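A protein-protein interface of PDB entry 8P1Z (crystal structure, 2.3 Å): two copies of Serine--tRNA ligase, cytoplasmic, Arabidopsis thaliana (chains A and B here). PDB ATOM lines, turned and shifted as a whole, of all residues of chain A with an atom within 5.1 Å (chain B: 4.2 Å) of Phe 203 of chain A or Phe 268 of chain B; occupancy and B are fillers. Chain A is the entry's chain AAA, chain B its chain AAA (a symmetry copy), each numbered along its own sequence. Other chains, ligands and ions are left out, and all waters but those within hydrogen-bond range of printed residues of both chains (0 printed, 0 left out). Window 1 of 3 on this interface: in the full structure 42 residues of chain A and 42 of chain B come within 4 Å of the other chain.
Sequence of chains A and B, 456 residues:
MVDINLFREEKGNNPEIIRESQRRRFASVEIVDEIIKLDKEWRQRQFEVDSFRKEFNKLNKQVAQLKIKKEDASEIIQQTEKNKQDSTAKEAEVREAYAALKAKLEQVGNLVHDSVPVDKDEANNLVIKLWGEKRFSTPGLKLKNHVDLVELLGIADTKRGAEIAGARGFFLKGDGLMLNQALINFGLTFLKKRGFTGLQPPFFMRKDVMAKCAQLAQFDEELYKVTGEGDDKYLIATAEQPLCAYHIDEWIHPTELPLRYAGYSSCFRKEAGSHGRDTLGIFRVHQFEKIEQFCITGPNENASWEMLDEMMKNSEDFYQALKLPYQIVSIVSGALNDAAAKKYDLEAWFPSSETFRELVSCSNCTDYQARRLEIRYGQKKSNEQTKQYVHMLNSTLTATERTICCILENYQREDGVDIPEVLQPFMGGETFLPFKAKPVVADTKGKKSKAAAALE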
ATOM      1  N   GLN A 200      20.206 -22.220  -4.546  1.00  0.00           N
ATOM      2  CA  GLN A 200      19.755 -21.244  -5.566  1.00  0.00           C
ATOM      3  C   GLN A 200      20.601 -20.003  -5.393  1.00  0.00           C
ATOM      4  O   GLN A 200      20.481 -19.314  -4.395  1.00  0.00           O
ATOM      5  CB  GLN A 200      18.268 -20.914  -5.446  1.00  0.00           C
ATOM      6  CG  GLN A 200      17.791 -19.833  -6.415  1.00  0.00           C
ATOM      7  CD  GLN A 200      16.290 -19.671  -6.384  1.00  0.00           C
ATOM      8  OE1 GLN A 200      15.559 -20.552  -5.932  1.00  0.00           O
ATOM      9  NE2 GLN A 200      15.812 -18.539  -6.872  1.00  0.00           N
ATOM     10  N   PRO A 201      21.490 -19.688  -6.351  1.00  0.00           N
ATOM     11  CA  PRO A 201      22.378 -18.551  -6.186  1.00  0.00           C
ATOM     12  C   PRO A 201      21.646 -17.280  -6.574  1.00  0.00           C
ATOM     13  O   PRO A 201      20.566 -17.336  -7.174  1.00  0.00           O
ATOM     14  CB  PRO A 201      23.486 -18.849  -7.187  1.00  0.00           C
ATOM     15  CG  PRO A 201      22.763 -19.543  -8.306  1.00  0.00           C
ATOM     16  CD  PRO A 201      21.692 -20.373  -7.633  1.00  0.00           C
ATOM     17  N   PRO A 202      22.235 -16.113  -6.245  1.00  0.00           N
ATOM     18  CA  PRO A 202      21.805 -14.852  -6.832  1.00  0.00           C
ATOM     19  C   PRO A 202      22.140 -14.912  -8.328  1.00  0.00           C
ATOM     20  O   PRO A 202      23.138 -15.519  -8.693  1.00  0.00           O
ATOM     21  CB  PRO A 202      22.617 -13.777  -6.110  1.00  0.00           C
ATOM     22  CG  PRO A 202      23.303 -14.484  -4.959  1.00  0.00           C
ATOM     23  CD  PRO A 202      23.357 -15.951  -5.314  1.00  0.00           C
ATOM     24  N   PHE A 203      21.297 -14.302  -9.154  1.00  0.00           N
ATOM     25  CA  PHE A 203      21.486 -14.237 -10.622  1.00  0.00           C
ATOM     26  C   PHE A 203      22.487 -13.127 -10.938  1.00  0.00           C
ATOM     27  O   PHE A 203      22.880 -13.020 -12.103  1.00  0.00           O
ATOM     28  CB  PHE A 203      20.158 -13.985 -11.337  1.00  0.00           C
ATOM     29  CG  PHE A 203      19.049 -14.960 -11.030  1.00  0.00           C
ATOM     30  CD1 PHE A 203      19.296 -16.177 -10.408  1.00  0.00           C
ATOM     31  CD2 PHE A 203      17.750 -14.668 -11.414  1.00  0.00           C
ATOM     32  CE1 PHE A 203      18.263 -17.064 -10.145  1.00  0.00           C
ATOM     33  CE2 PHE A 203      16.721 -15.566 -11.173  1.00  0.00           C
ATOM     34  CZ  PHE A 203      16.977 -16.761 -10.535  1.00  0.00           C
ATOM     35  N   PHE A 204      22.848 -12.318  -9.935  1.00  0.00           N
ATOM     36  CA  PHE A 204      23.932 -11.307 -10.009  1.00  0.00           C
ATOM     37  C   PHE A 204      25.247 -11.951  -9.584  1.00  0.00           C
ATOM     38  O   PHE A 204      25.237 -12.876  -8.746  1.00  0.00           O
ATOM     39  CB  PHE A 204      23.705 -10.139  -9.049  1.00  0.00           C
ATOM     40  CG  PHE A 204      22.544  -9.244  -9.380  1.00  0.00           C
ATOM     41  CD1 PHE A 204      21.771  -9.449 -10.513  1.00  0.00           C
ATOM     42  CD2 PHE A 204      22.227  -8.186  -8.543  1.00  0.00           C
ATOM     43  CE1 PHE A 204      20.701  -8.617 -10.800  1.00  0.00           C
ATOM     44  CE2 PHE A 204      21.153  -7.359  -8.827  1.00  0.00           C
ATOM     45  CZ  PHE A 204      20.396  -7.574  -9.958  1.00  0.00           C
ATOM     46  N   MET A 205      26.350 -11.430 -10.118  1.00  0.00           N
ATOM     47  CA  MET A 205      27.712 -11.759  -9.644  1.00  0.00           C
ATOM     48  C   MET A 205      28.678 -10.647 -10.051  1.00  0.00           C
ATOM     49  O   MET A 205      28.626 -10.182 -11.205  1.00  0.00           O
ATOM     50  CB  MET A 205      28.188 -13.098 -10.206  1.00  0.00           C
ATOM     51  CG  MET A 205      29.509 -13.543  -9.615  1.00  0.00           C
ATOM     52  SD  MET A 205      30.020 -15.210 -10.087  1.00  0.00           S
ATOM     53  CE  MET A 205      28.438 -15.920 -10.520  1.00  0.00           C
ATOM     54  N   TYR A 234      27.495  -8.892 -13.534  1.00  0.00           N
ATOM     55  CA  TYR A 234      26.995  -9.695 -14.674  1.00  0.00           C
ATOM     56  C   TYR A 234      25.753 -10.480 -14.253  1.00  0.00           C
ATOM     57  O   TYR A 234      25.698 -10.929 -13.101  1.00  0.00           O
ATOM     58  CB  TYR A 234      28.016 -10.736 -15.124  1.00  0.00           C
ATOM     59  CG  TYR A 234      29.357 -10.233 -15.600  1.00  0.00           C
ATOM     60  CD1 TYR A 234      29.491  -9.409 -16.714  1.00  0.00           C
ATOM     61  CD2 TYR A 234      30.515 -10.678 -14.980  1.00  0.00           C
ATOM     62  CE1 TYR A 234      30.739  -9.006 -17.166  1.00  0.00           C
ATOM     63  CE2 TYR A 234      31.767 -10.285 -15.419  1.00  0.00           C
ATOM     64  CZ  TYR A 234      31.879  -9.446 -16.510  1.00  0.00           C
ATOM     65  OH  TYR A 234      33.131  -9.082 -16.900  1.00  0.00           O
ATOM     66  N   LEU A 235      24.823 -10.681 -15.188  1.00  0.00           N
ATOM     67  CA  LEU A 235      23.847 -11.799 -15.138  1.00  0.00           C
ATOM     68  C   LEU A 235      24.571 -13.127 -15.418  1.00  0.00           C
ATOM     69  O   LEU A 235      25.415 -13.202 -16.352  1.00  0.00           O
ATOM     70  CB  LEU A 235      22.732 -11.546 -16.154  1.00  0.00           C
ATOM     71  CG  LEU A 235      21.687 -10.507 -15.755  1.00  0.00           C
ATOM     72  CD1 LEU A 235      20.795 -10.161 -16.931  1.00  0.00           C
ATOM     73  CD2 LEU A 235      20.832 -10.994 -14.598  1.00  0.00           C
ATOM     74  N   ILE A 236      24.246 -14.160 -14.648  1.00  0.00           N
ATOM     75  CA  ILE A 236      24.894 -15.501 -14.772  1.00  0.00           C
ATOM     76  C   ILE A 236      24.380 -16.243 -16.014  1.00  0.00           C
ATOM     77  O   ILE A 236      23.156 -16.225 -16.275  1.00  0.00           O
ATOM     78  CB  ILE A 236      24.702 -16.325 -13.486  1.00  0.00           C
ATOM     79  CG1 ILE A 236      23.230 -16.655 -13.202  1.00  0.00           C
ATOM     80  CG2 ILE A 236      25.369 -15.596 -12.333  1.00  0.00           C
ATOM     81  CD1 ILE A 236      23.015 -17.633 -12.070  1.00  0.00           C
ATOM     82  N   SER A 265      18.867 -22.197 -10.941  1.00  0.00           N
ATOM     83  CA  SER A 265      18.735 -20.755 -11.285  1.00  0.00           C
ATOM     84  C   SER A 265      18.181 -20.550 -12.692  1.00  0.00           C
ATOM     85  O   SER A 265      18.277 -21.473 -13.524  1.00  0.00           O
ATOM     86  CB  SER A 265      20.039 -20.023 -11.159  1.00  0.00           C
ATOM     87  OG  SER A 265      21.003 -20.556 -12.039  1.00  0.00           O
ATOM     88  N   SER A 266      17.633 -19.353 -12.921  1.00  0.00           N
ATOM     89  CA  SER A 266      17.530 -18.705 -14.248  1.00  0.00           C
ATOM     90  C   SER A 266      18.951 -18.475 -14.784  1.00  0.00           C
ATOM     91  O   SER A 266      19.909 -18.359 -13.969  1.00  0.00           O
ATOM     92  CB  SER A 266      16.745 -17.422 -14.185  1.00  0.00           C
ATOM     93  OG  SER A 266      15.347 -17.684 -14.148  1.00  0.00           O
ATOM     94  N   PHE A 268      21.153 -16.453 -18.232  1.00  0.00           N
ATOM     95  CA  PHE A 268      21.139 -15.353 -19.222  1.00  0.00           C
ATOM     96  C   PHE A 268      22.370 -15.525 -20.112  1.00  0.00           C
ATOM     97  O   PHE A 268      23.507 -15.431 -19.605  1.00  0.00           O
ATOM     98  CB  PHE A 268      21.044 -14.017 -18.481  1.00  0.00           C
ATOM     99  CG  PHE A 268      19.953 -14.016 -17.439  1.00  0.00           C
ATOM    100  CD1 PHE A 268      20.204 -14.474 -16.147  1.00  0.00           C
ATOM    101  CD2 PHE A 268      18.662 -13.622 -17.763  1.00  0.00           C
ATOM    102  CE1 PHE A 268      19.193 -14.526 -15.200  1.00  0.00           C
ATOM    103  CE2 PHE A 268      17.649 -13.682 -16.815  1.00  0.00           C
ATOM    104  CZ  PHE A 268      17.918 -14.129 -15.535  1.00  0.00           C
ATOM    105  N   PHE B 203      12.158 -11.657 -17.684  1.00  0.00           N
ATOM    106  CA  PHE B 203      12.619 -10.746 -16.610  1.00  0.00           C
ATOM    107  C   PHE B 203      13.198  -9.487 -17.252  1.00  0.00           C
ATOM    108  O   PHE B 203      13.501  -8.549 -16.509  1.00  0.00           O
ATOM    109  CB  PHE B 203      13.662 -11.427 -15.722  1.00  0.00           C
ATOM    110  CG  PHE B 203      13.246 -12.738 -15.104  1.00  0.00           C
ATOM    111  CD1 PHE B 203      11.918 -13.143 -15.071  1.00  0.00           C
ATOM    112  CD2 PHE B 203      14.197 -13.551 -14.511  1.00  0.00           C
ATOM    113  CE1 PHE B 203      11.556 -14.348 -14.489  1.00  0.00           C
ATOM    114  CE2 PHE B 203      13.833 -14.745 -13.906  1.00  0.00           C
ATOM    115  CZ  PHE B 203      12.513 -15.145 -13.899  1.00  0.00           C
ATOM    116  N   LEU B 223      15.007   1.065 -11.326  1.00  0.00           N
ATOM    117  CA  LEU B 223      15.200  -0.333 -11.785  1.00  0.00           C
ATOM    118  C   LEU B 223      16.653  -0.521 -12.212  1.00  0.00           C
ATOM    119  O   LEU B 223      17.340   0.483 -12.483  1.00  0.00           O
ATOM    120  CB  LEU B 223      14.272  -0.597 -12.973  1.00  0.00           C
ATOM    121  CG  LEU B 223      12.784  -0.482 -12.669  1.00  0.00           C
ATOM    122  CD1 LEU B 223      11.965  -0.419 -13.947  1.00  0.00           C
ATOM    123  CD2 LEU B 223      12.334  -1.635 -11.793  1.00  0.00           C
ATOM    124  N   TYR B 224      17.073  -1.774 -12.307  1.00  0.00           N
ATOM    125  CA  TYR B 224      18.353  -2.193 -12.922  1.00  0.00           C
ATOM    126  C   TYR B 224      18.225  -2.059 -14.444  1.00  0.00           C
ATOM    127  O   TYR B 224      17.147  -2.394 -14.984  1.00  0.00           O
ATOM    128  CB  TYR B 224      18.678  -3.632 -12.516  1.00  0.00           C
ATOM    129  CG  TYR B 224      18.991  -3.842 -11.052  1.00  0.00           C
ATOM    130  CD1 TYR B 224      20.296  -3.729 -10.591  1.00  0.00           C
ATOM    131  CD2 TYR B 224      17.997  -4.163 -10.130  1.00  0.00           C
ATOM    132  CE1 TYR B 224      20.607  -3.928  -9.257  1.00  0.00           C
ATOM    133  CE2 TYR B 224      18.295  -4.347  -8.791  1.00  0.00           C
ATOM    134  CZ  TYR B 224      19.604  -4.241  -8.358  1.00  0.00           C
ATOM    135  OH  TYR B 224      19.941  -4.445  -7.054  1.00  0.00           O
ATOM    136  N   LEU B 235      15.606  -4.816 -15.879  1.00  0.00           N
ATOM    137  CA  LEU B 235      15.098  -5.923 -15.029  1.00  0.00           C
ATOM    138  C   LEU B 235      13.768  -5.506 -14.381  1.00  0.00           C
ATOM    139  O   LEU B 235      13.641  -4.355 -13.882  1.00  0.00           O
ATOM    140  CB  LEU B 235      16.148  -6.275 -13.973  1.00  0.00           C
ATOM    141  CG  LEU B 235      17.343  -7.089 -14.463  1.00  0.00           C
ATOM    142  CD1 LEU B 235      18.423  -7.153 -13.401  1.00  0.00           C
ATOM    143  CD2 LEU B 235      16.933  -8.498 -14.854  1.00  0.00           C
ATOM    144  N   ILE B 236      12.798  -6.414 -14.366  1.00  0.00           N
ATOM    145  CA  ILE B 236      11.437  -6.142 -13.810  1.00  0.00           C
ATOM    146  C   ILE B 236      11.469  -6.125 -12.276  1.00  0.00           C
ATOM    147  O   ILE B 236      12.119  -7.004 -11.666  1.00  0.00           O
ATOM    148  CB  ILE B 236      10.410  -7.149 -14.356  1.00  0.00           C
ATOM    149  CG1 ILE B 236      10.699  -8.593 -13.923  1.00  0.00           C
ATOM    150  CG2 ILE B 236      10.330  -6.998 -15.865  1.00  0.00           C
ATOM    151  CD1 ILE B 236       9.605  -9.579 -14.261  1.00  0.00           C
ATOM    152  N   ALA B 237      10.758  -5.159 -11.690  1.00  0.00           N
ATOM    153  CA  ALA B 237      10.513  -5.032 -10.231  1.00  0.00           C
ATOM    154  C   ALA B 237       9.338  -5.925  -9.823  1.00  0.00           C
ATOM    155  O   ALA B 237       9.281  -6.308  -8.654  1.00  0.00           O
ATOM    156  CB  ALA B 237      10.240  -3.594  -9.862  1.00  0.00           C
ATOM    157  N   SER B 266      10.870 -14.034 -10.914  1.00  0.00           N
ATOM    158  CA  SER B 266      11.898 -13.294 -10.148  1.00  0.00           C
ATOM    159  C   SER B 266      11.633 -11.790 -10.313  1.00  0.00           C
ATOM    160  O   SER B 266      11.028 -11.377 -11.343  1.00  0.00           O
ATOM    161  CB  SER B 266      13.292 -13.663 -10.581  1.00  0.00           C
ATOM    162  OG  SER B 266      13.688 -14.905 -10.010  1.00  0.00           O
ATOM    163  N   CYS B 267      12.057 -11.008  -9.321  1.00  0.00           N
ATOM    164  CA  CYS B 267      11.872  -9.540  -9.243  1.00  0.00           C
ATOM    165  C   CYS B 267      13.171  -8.906  -8.776  1.00  0.00           C
ATOM    166  O   CYS B 267      13.848  -9.511  -7.942  1.00  0.00           O
ATOM    167  CB  CYS B 267      10.768  -9.172  -8.267  1.00  0.00           C
ATOM    168  SG  CYS B 267       9.164  -9.862  -8.728  1.00  0.00           S
ATOM    169  N   PHE B 268      13.481  -7.737  -9.322  1.00  0.00           N
ATOM    170  CA  PHE B 268      14.731  -6.983  -9.080  1.00  0.00           C
ATOM    171  C   PHE B 268      14.337  -5.556  -8.698  1.00  0.00           C
ATOM    172  O   PHE B 268      13.736  -4.845  -9.530  1.00  0.00           O
ATOM    173  CB  PHE B 268      15.634  -7.108 -10.310  1.00  0.00           C
ATOM    174  CG  PHE B 268      15.772  -8.536 -10.776  1.00  0.00           C
ATOM    175  CD1 PHE B 268      14.848  -9.089 -11.659  1.00  0.00           C
ATOM    176  CD2 PHE B 268      16.785  -9.348 -10.283  1.00  0.00           C
ATOM    177  CE1 PHE B 268      14.939 -10.417 -12.049  1.00  0.00           C
ATOM    178  CE2 PHE B 268      16.871 -10.679 -10.668  1.00  0.00           C
ATOM    179  CZ  PHE B 268      15.951 -11.209 -11.554  1.00  0.00           C
ATOM    180  N   ARG B 269      14.594  -5.203  -7.438  1.00  0.00           N
ATOM    181  CA  ARG B 269      14.333  -3.867  -6.833  1.00  0.00           C
ATOM    182  C   ARG B 269      15.697  -3.304  -6.413  1.00  0.00           C
ATOM    183  O   ARG B 269      16.482  -4.052  -5.782  1.00  0.00           O
ATOM    184  CB  ARG B 269      13.343  -3.993  -5.663  1.00  0.00           C
ATOM    185  CG  ARG B 269      12.390  -2.815  -5.478  1.00  0.00           C
ATOM    186  CD  ARG B 269      11.517  -2.901  -4.220  1.00  0.00           C
ATOM    187  NE  ARG B 269      11.482  -1.652  -3.444  1.00  0.00           N
ATOM    188  CZ  ARG B 269      10.455  -0.794  -3.349  1.00  0.00           C
ATOM    189  NH1 ARG B 269      10.577   0.298  -2.608  1.00  0.00           N
ATOM    190  NH2 ARG B 269       9.311  -1.019  -3.975  1.00  0.00           N
ATOM    191  N   HIS B 286      17.411  -7.392  -2.815  1.00  0.00           N
ATOM    192  CA  HIS B 286      17.458  -6.895  -4.220  1.00  0.00           C
ATOM    193  C   HIS B 286      16.751  -7.841  -5.199  1.00  0.00           C
ATOM    194  O   HIS B 286      16.260  -7.326  -6.209  1.00  0.00           O
ATOM    195  CB  HIS B 286      18.901  -6.678  -4.670  1.00  0.00           C
ATOM    196  CG  HIS B 286      19.552  -5.512  -4.011  1.00  0.00           C
ATOM    197  ND1 HIS B 286      19.020  -4.231  -4.058  1.00  0.00           N
ATOM    198  CD2 HIS B 286      20.699  -5.431  -3.311  1.00  0.00           C
ATOM    199  CE1 HIS B 286      19.820  -3.413  -3.412  1.00  0.00           C
ATOM    200  NE2 HIS B 286      20.855  -4.130  -2.935  1.00  0.00           N
ATOM    201  N   GLN B 287      16.745  -9.157  -4.943  1.00  0.00           N
ATOM    202  CA  GLN B 287      16.151 -10.184  -5.844  1.00  0.00           C
ATOM    203  C   GLN B 287      15.197 -11.077  -5.052  1.00  0.00           C
ATOM    204  O   GLN B 287      15.597 -11.566  -3.992  1.00  0.00           O
ATOM    205  CB  GLN B 287      17.245 -11.051  -6.475  1.00  0.00           C
ATOM    206  CG  GLN B 287      16.699 -12.191  -7.328  1.00  0.00           C
ATOM    207  CD  GLN B 287      17.729 -13.220  -7.732  1.00  0.00           C
ATOM    208  OE1 GLN B 287      17.382 -14.339  -8.108  1.00  0.00           O
ATOM    209  NE2 GLN B 287      18.998 -12.851  -7.668  1.00  0.00           N
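O of Phe 203 of chain A is in hydrogen-bond range of N of Ile 236 of chain A (3.1 Å). O of Ile 236 of chain A is in hydrogen-bond range of N of Phe 268 of chain A (2.8 Å). The backbone carbonyl oxygen (O) of Phe 203 of chain B is in hydrogen-bond range of the backbone NH (N) of Ile 236 of chain B (3.1 Å). The backbone carbonyl oxygen (O) of Tyr 224 of chain B is in hydrogen-bond range of the backbone NH (N) of Leu 235 of chain B, 3.0 Å away. The side-chain hydroxyl (OH) of Tyr 224 of chain B lies within hydrogen-bond range of a ring nitrogen (ND1) of His 286 of chain B (3.1 Å). The backbone NH of Phe 268 of chain B sits at hydrogen-bond distance from the backbone carbonyl oxygen of Ile 236 of chain B (2.8 Å).
Of the 12 printed residues of chain A, 5 touch a printed residue of chain B. Of the 12 printed residues of chain B, 6 touch a printed residue of chain A.
Of the printed residues of chain B, Phe 203 of chain A touches Ser 266 (3.3 Å), Phe 268 (3.9 Å) and Gln 287 (3.1 Å). Of the printed residues of chain A, Phe 268 of chain B touches Phe 203 (3.9 Å). Printed residues of chain B within 4 Å of Pro 202 of chain A: Gln 287. Printed residues of chain B within 4 Å of Ser 266 of chain A: Phe 203. Of the printed residues of chain A, Leu 235 of chain B touches Phe 204. The nearest printed residue of chain A that does not touch Phe 268 of chain B is Phe 204 of chain A (4.02 Å).
The backbone NH of Phe 203 of chain A sits close to the side-chain amide nitrogen of Gln 287 of chain B, 3.1 Å away.
Phe 203 of chain A touches Ser 266 of chain B, and with the chains exchanged Ser 266 of chain A touches Phe 203 of chain B. Phe 203 of chain A touches Phe 268 of chain B, and with the chains exchanged Phe 268 of chain A touches Phe 203 of chain B. Positions printed for both chains: 203, 235, 236, 266 and 268. Of the 8 pairs that touch across the chains among the printed residues, 4 have their exchanged pair printed and touching as well.
Pro 202 of chain A touches Gln 287 of chain B. Ser 266 of chain B touches Phe 203 of chain A. Phe 203 of chain A touches Phe 268 of chain B (CD2 to CZ, 3.9 Å). Phe 204 of chain A touches Tyr 224 of chain B. CE1 of Phe 204 of chain A touches CD1 of Leu 235 of chain B, 3.8 Å away. Ser 266 of chain A touches Phe 203 of chain B. Phe 203 of chain B touches Phe 268 of chain A.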
